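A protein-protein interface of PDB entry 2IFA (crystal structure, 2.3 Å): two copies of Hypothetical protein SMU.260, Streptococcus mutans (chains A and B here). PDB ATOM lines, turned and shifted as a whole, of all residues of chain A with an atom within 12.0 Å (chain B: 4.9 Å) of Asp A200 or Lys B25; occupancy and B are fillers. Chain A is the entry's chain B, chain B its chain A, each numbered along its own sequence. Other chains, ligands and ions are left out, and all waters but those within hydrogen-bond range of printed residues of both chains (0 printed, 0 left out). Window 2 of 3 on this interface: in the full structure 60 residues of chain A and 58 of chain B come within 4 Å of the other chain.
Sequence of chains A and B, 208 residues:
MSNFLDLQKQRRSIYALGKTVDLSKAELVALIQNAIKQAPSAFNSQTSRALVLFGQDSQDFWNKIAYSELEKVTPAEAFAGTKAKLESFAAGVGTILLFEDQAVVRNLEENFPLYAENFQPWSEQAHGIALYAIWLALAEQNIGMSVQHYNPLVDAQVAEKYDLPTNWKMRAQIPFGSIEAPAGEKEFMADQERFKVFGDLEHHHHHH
The backbone NH (N) of Gly B55 is in hydrogen-bond range of the backbone carbonyl oxygen (O) of Asp A200 (3.1 Å).
The side-chain amino group (NZ) of Lys B25 sits at hydrogen-bond distance from the backbone carbonyl oxygen (O) of Gly A199 (2.6 Å).
The backbone carbonyl oxygen of Phe A198 is in hydrogen-bond range of the backbone NH of Phe B54.
The side-chain carboxylate (OD1) of Asp A200 is in salt-bridge range of the side-chain amino group (NZ) of Lys B25, 3.5 Å away.
N of Ser B24 sits at hydrogen-bond distance from OE1 of Glu B27 (3.2 Å).
CG1 of Val A197 touches CE of Lys B25 (3.6 Å).
Val B29 touches Val A197 (CG2 to CG1, 3.96 Å).
Phe B54 touches Gly A199.
Asp A200 touches Phe B54 (N to CB, 3.5 Å).
Leu A201 touches Leu B23 (CD2 to O, 3.5 Å).
Leu A201 touches Ser B24.
CB of Lys B25 touches CD1 of Leu A201 (3.5 Å).
CD1 of Leu A201 touches CD1 of Phe B54, 3.7 Å away.
Of chain B, only Lys B25, Phe B54 and Gly B55 come within 4 Å of Asp A200.
Ser B24 touches one residue of chain A.
No residue of chain A comes within 4 Å of Glu B27.
No residue of chain A comes within 4 Å of Leu B28.
Printed residues of chain A within 4 Å of Phe B54: Phe A198 (2.8 Å), Gly A199 (3.5 Å), Asp A200 (3.5 Å) and Leu A201 (3.7 Å).
Printed residues of chain B within 4 Å of Phe A198: Phe B54.
Printed residues of chain A within 4 Å of Leu B23: Leu A201.
Of the printed residues of chain B, Val A197 touches Lys B25 (3.6 Å) and Val B29 (3.96 Å).
Of the printed residues of chain B, Gly A199 touches Lys B25 and Phe B54.
Printed residues of chain B within 4 Å of Leu A201: Leu B23, Ser B24, Lys B25 and Phe B54.
The nearest printed residue of chain B that does not touch Asp A200 is Leu B28 (8.2 Å).
The nearest printed residue of chain B that does not touch Gly A199 is Gly B55 (4.8 Å).
Hydrophobic or aromatic side chains of chain A within 4 Å of the printed part of chain B: Val A197 and Leu A201.
Hydrophobic or aromatic side chains of chain B within 4 Å of the printed part of chain A: Val B29 and Phe B54.
Along chain B the printed residues that touch a printed residue of chain A span positions 23 to 55.
No position is printed for both chains.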
ATOM      1  N   PHE A 195      29.979 -26.922  10.317  1.00  0.00           N
ATOM      2  CA  PHE A 195      29.064 -25.964  10.924  1.00  0.00           C
ATOM      3  C   PHE A 195      27.746 -25.786  10.165  1.00  0.00           C
ATOM      4  O   PHE A 195      27.626 -26.191   9.014  1.00  0.00           O
ATOM      5  CB  PHE A 195      29.726 -24.578  11.004  1.00  0.00           C
ATOM      6  CG  PHE A 195      31.101 -24.570  11.632  1.00  0.00           C
ATOM      7  CD1 PHE A 195      31.272 -24.862  12.976  1.00  0.00           C
ATOM      8  CD2 PHE A 195      32.222 -24.241  10.874  1.00  0.00           C
ATOM      9  CE1 PHE A 195      32.533 -24.826  13.566  1.00  0.00           C
ATOM     10  CE2 PHE A 195      33.497 -24.206  11.451  1.00  0.00           C
ATOM     11  CZ  PHE A 195      33.649 -24.502  12.807  1.00  0.00           C
ATOM     12  N   LYS A 196      26.772 -25.169  10.843  1.00  0.00           N
ATOM     13  CA  LYS A 196      25.467 -24.823  10.264  1.00  0.00           C
ATOM     14  C   LYS A 196      24.956 -23.564  10.988  1.00  0.00           C
ATOM     15  O   LYS A 196      25.087 -23.450  12.219  1.00  0.00           O
ATOM     16  CB  LYS A 196      24.436 -25.943  10.437  1.00  0.00           C
ATOM     17  CG  LYS A 196      24.697 -27.214   9.643  1.00  0.00           C
ATOM     18  CD  LYS A 196      23.560 -28.217   9.889  1.00  0.00           C
ATOM     19  CE  LYS A 196      23.890 -29.617   9.411  1.00  0.00           C
ATOM     20  NZ  LYS A 196      24.453 -29.649   8.043  1.00  0.00           N
ATOM     21  N   VAL A 197      24.384 -22.628  10.227  1.00  0.00           N
ATOM     22  CA  VAL A 197      23.870 -21.384  10.791  1.00  0.00           C
ATOM     23  C   VAL A 197      22.417 -21.124  10.366  1.00  0.00           C
ATOM     24  O   VAL A 197      22.089 -21.179   9.192  1.00  0.00           O
ATOM     25  CB  VAL A 197      24.750 -20.179  10.356  1.00  0.00           C
ATOM     26  CG1 VAL A 197      24.212 -18.880  10.959  1.00  0.00           C
ATOM     27  CG2 VAL A 197      26.196 -20.411  10.786  1.00  0.00           C
ATOM     28  N   PHE A 198      21.555 -20.825  11.334  1.00  0.00           N
ATOM     29  CA  PHE A 198      20.138 -20.577  11.065  1.00  0.00           C
ATOM     30  C   PHE A 198      19.639 -19.336  11.811  1.00  0.00           C
ATOM     31  O   PHE A 198      19.911 -19.170  12.990  1.00  0.00           O
ATOM     32  CB  PHE A 198      19.303 -21.778  11.504  1.00  0.00           C
ATOM     33  CG  PHE A 198      19.529 -22.997  10.679  1.00  0.00           C
ATOM     34  CD1 PHE A 198      18.757 -23.239   9.547  1.00  0.00           C
ATOM     35  CD2 PHE A 198      20.530 -23.902  11.010  1.00  0.00           C
ATOM     36  CE1 PHE A 198      18.982 -24.365   8.757  1.00  0.00           C
ATOM     37  CE2 PHE A 198      20.760 -25.032  10.221  1.00  0.00           C
ATOM     38  CZ  PHE A 198      19.982 -25.259   9.096  1.00  0.00           C
ATOM     39  N   GLY A 199      18.894 -18.481  11.116  1.00  0.00           N
ATOM     40  CA  GLY A 199      18.361 -17.287  11.740  1.00  0.00           C
ATOM     41  C   GLY A 199      19.175 -16.040  11.435  1.00  0.00           C
ATOM     42  O   GLY A 199      20.257 -16.126  10.876  1.00  0.00           O
ATOM     43  N   ASP A 200      18.636 -14.883  11.812  1.00  0.00           N
ATOM     44  CA  ASP A 200      19.287 -13.590  11.585  1.00  0.00           C
ATOM     45  C   ASP A 200      19.098 -12.715  12.822  1.00  0.00           C
ATOM     46  O   ASP A 200      18.216 -12.969  13.639  1.00  0.00           O
ATOM     47  CB  ASP A 200      18.652 -12.864  10.392  1.00  0.00           C
ATOM     48  CG  ASP A 200      18.114 -13.823   9.332  1.00  0.00           C
ATOM     49  OD1 ASP A 200      18.908 -14.313   8.496  1.00  0.00           O
ATOM     50  OD2 ASP A 200      16.888 -14.087   9.347  1.00  0.00           O
ATOM     51  N   LEU A 201      19.931 -11.688  12.956  1.00  0.00           N
ATOM     52  CA  LEU A 201      19.830 -10.761  14.076  1.00  0.00           C
ATOM     53  C   LEU A 201      18.567  -9.909  13.912  1.00  0.00           C
ATOM     54  O   LEU A 201      18.100  -9.680  12.790  1.00  0.00           O
ATOM     55  CB  LEU A 201      21.053  -9.842  14.124  1.00  0.00           C
ATOM     56  CG  LEU A 201      22.332 -10.289  14.834  1.00  0.00           C
ATOM     57  CD1 LEU A 201      22.883 -11.574  14.227  1.00  0.00           C
ATOM     58  CD2 LEU A 201      23.351  -9.169  14.723  1.00  0.00           C
ATOM     59  N   GLU A 202      18.019  -9.450  15.033  1.00  0.00           N
ATOM     60  CA  GLU A 202      16.821  -8.620  15.025  1.00  0.00           C
ATOM     61  C   GLU A 202      17.134  -7.214  14.496  1.00  0.00           C
ATOM     62  O   GLU A 202      16.311  -6.676  13.728  1.00  0.00           O
ATOM     63  CB  GLU A 202      16.234  -8.518  16.436  1.00  0.00           C
ATOM     64  CG  GLU A 202      17.199  -7.924  17.457  1.00  0.00           C
ATOM     65  CD  GLU A 202      16.507  -7.030  18.483  1.00  0.00           C
ATOM     66  OE1 GLU A 202      17.202  -6.547  19.404  1.00  0.00           O
ATOM     67  OE2 GLU A 202      15.279  -6.804  18.366  1.00  0.00           O
ATOM     68  N   LEU B  23      28.221  -6.465  17.251  1.00  0.00           N
ATOM     69  CA  LEU B  23      28.760  -7.225  16.125  1.00  0.00           C
ATOM     70  C   LEU B  23      27.633  -7.753  15.241  1.00  0.00           C
ATOM     71  O   LEU B  23      26.541  -8.031  15.728  1.00  0.00           O
ATOM     72  CB  LEU B  23      29.602  -8.394  16.628  1.00  0.00           C
ATOM     73  CG  LEU B  23      30.901  -8.054  17.360  1.00  0.00           C
ATOM     74  CD1 LEU B  23      31.565  -9.343  17.775  1.00  0.00           C
ATOM     75  CD2 LEU B  23      31.834  -7.231  16.461  1.00  0.00           C
ATOM     76  N   SER B  24      27.894  -7.885  13.944  1.00  0.00           N
ATOM     77  CA  SER B  24      26.879  -8.397  13.022  1.00  0.00           C
ATOM     78  C   SER B  24      26.866  -9.927  13.031  1.00  0.00           C
ATOM     79  O   SER B  24      27.660 -10.561  13.741  1.00  0.00           O
ATOM     80  CB  SER B  24      27.160  -7.914  11.599  1.00  0.00           C
ATOM     81  OG  SER B  24      28.375  -8.465  11.116  1.00  0.00           O
ATOM     82  N   LYS B  25      25.974 -10.512  12.234  1.00  0.00           N
ATOM     83  CA  LYS B  25      25.860 -11.966  12.138  1.00  0.00           C
ATOM     84  C   LYS B  25      27.123 -12.555  11.528  1.00  0.00           C
ATOM     85  O   LYS B  25      27.648 -13.565  12.005  1.00  0.00           O
ATOM     86  CB  LYS B  25      24.655 -12.353  11.277  1.00  0.00           C
ATOM     87  CG  LYS B  25      24.488 -13.848  11.052  1.00  0.00           C
ATOM     88  CD  LYS B  25      23.309 -14.137  10.120  1.00  0.00           C
ATOM     89  CE  LYS B  25      23.147 -15.640   9.835  1.00  0.00           C
ATOM     90  NZ  LYS B  25      21.966 -15.972   8.965  1.00  0.00           N
ATOM     91  N   ALA B  26      27.605 -11.925  10.466  1.00  0.00           N
ATOM     92  CA  ALA B  26      28.808 -12.394   9.802  1.00  0.00           C
ATOM     93  C   ALA B  26      30.013 -12.397  10.762  1.00  0.00           C
ATOM     94  O   ALA B  26      30.823 -13.320  10.748  1.00  0.00           O
ATOM     95  CB  ALA B  26      29.097 -11.524   8.584  1.00  0.00           C
ATOM     96  N   GLU B  27      30.124 -11.371  11.599  1.00  0.00           N
ATOM     97  CA  GLU B  27      31.241 -11.270  12.545  1.00  0.00           C
ATOM     98  C   GLU B  27      31.086 -12.238  13.717  1.00  0.00           C
ATOM     99  O   GLU B  27      32.074 -12.735  14.259  1.00  0.00           O
ATOM    100  CB  GLU B  27      31.355  -9.835  13.059  1.00  0.00           C
ATOM    101  CG  GLU B  27      31.592  -8.789  11.961  1.00  0.00           C
ATOM    102  CD  GLU B  27      31.786  -7.398  12.534  1.00  0.00           C
ATOM    103  OE1 GLU B  27      30.907  -6.946  13.298  1.00  0.00           O
ATOM    104  OE2 GLU B  27      32.818  -6.763  12.231  1.00  0.00           O
ATOM    105  N   LEU B  28      29.844 -12.491  14.112  1.00  0.00           N
ATOM    106  CA  LEU B  28      29.570 -13.415  15.202  1.00  0.00           C
ATOM    107  C   LEU B  28      29.853 -14.835  14.709  1.00  0.00           C
ATOM    108  O   LEU B  28      30.506 -15.625  15.404  1.00  0.00           O
ATOM    109  CB  LEU B  28      28.108 -13.282  15.667  1.00  0.00           C
ATOM    110  CG  LEU B  28      27.792 -12.018  16.487  1.00  0.00           C
ATOM    111  CD1 LEU B  28      26.281 -11.864  16.711  1.00  0.00           C
ATOM    112  CD2 LEU B  28      28.533 -12.100  17.814  1.00  0.00           C
ATOM    113  N   VAL B  29      29.382 -15.155  13.506  1.00  0.00           N
ATOM    114  CA  VAL B  29      29.613 -16.475  12.936  1.00  0.00           C
ATOM    115  C   VAL B  29      31.111 -16.759  12.754  1.00  0.00           C
ATOM    116  O   VAL B  29      31.611 -17.812  13.146  1.00  0.00           O
ATOM    117  CB  VAL B  29      28.918 -16.616  11.583  1.00  0.00           C
ATOM    118  CG1 VAL B  29      29.412 -17.847  10.866  1.00  0.00           C
ATOM    119  CG2 VAL B  29      27.414 -16.698  11.788  1.00  0.00           C
ATOM    120  N   ALA B  30      31.832 -15.821  12.159  1.00  0.00           N
ATOM    121  CA  ALA B  30      33.255 -16.040  11.948  1.00  0.00           C
ATOM    122  C   ALA B  30      34.016 -16.158  13.275  1.00  0.00           C
ATOM    123  O   ALA B  30      34.962 -16.923  13.379  1.00  0.00           O
ATOM    124  CB  ALA B  30      33.840 -14.918  11.102  1.00  0.00           C
ATOM    125  N   PHE B  54      20.186 -17.896  15.462  1.00  0.00           N
ATOM    126  CA  PHE B  54      19.937 -16.469  15.664  1.00  0.00           C
ATOM    127  C   PHE B  54      18.445 -16.170  15.592  1.00  0.00           C
ATOM    128  O   PHE B  54      17.641 -17.017  15.168  1.00  0.00           O
ATOM    129  CB  PHE B  54      20.663 -15.628  14.607  1.00  0.00           C
ATOM    130  CG  PHE B  54      22.147 -15.591  14.782  1.00  0.00           C
ATOM    131  CD1 PHE B  54      22.719 -14.891  15.840  1.00  0.00           C
ATOM    132  CD2 PHE B  54      22.979 -16.266  13.897  1.00  0.00           C
ATOM    133  CE1 PHE B  54      24.103 -14.865  16.012  1.00  0.00           C
ATOM    134  CE2 PHE B  54      24.362 -16.245  14.063  1.00  0.00           C
ATOM    135  CZ  PHE B  54      24.923 -15.546  15.119  1.00  0.00           C
ATOM    136  N   GLY B  55      18.091 -14.958  16.011  1.00  0.00           N
ATOM    137  CA  GLY B  55      16.709 -14.514  15.976  1.00  0.00           C
ATOM    138  C   GLY B  55      15.691 -15.489  16.529  1.00  0.00           C
ATOM    139  O   GLY B  55      15.881 -16.071  17.605  1.00  0.00           O
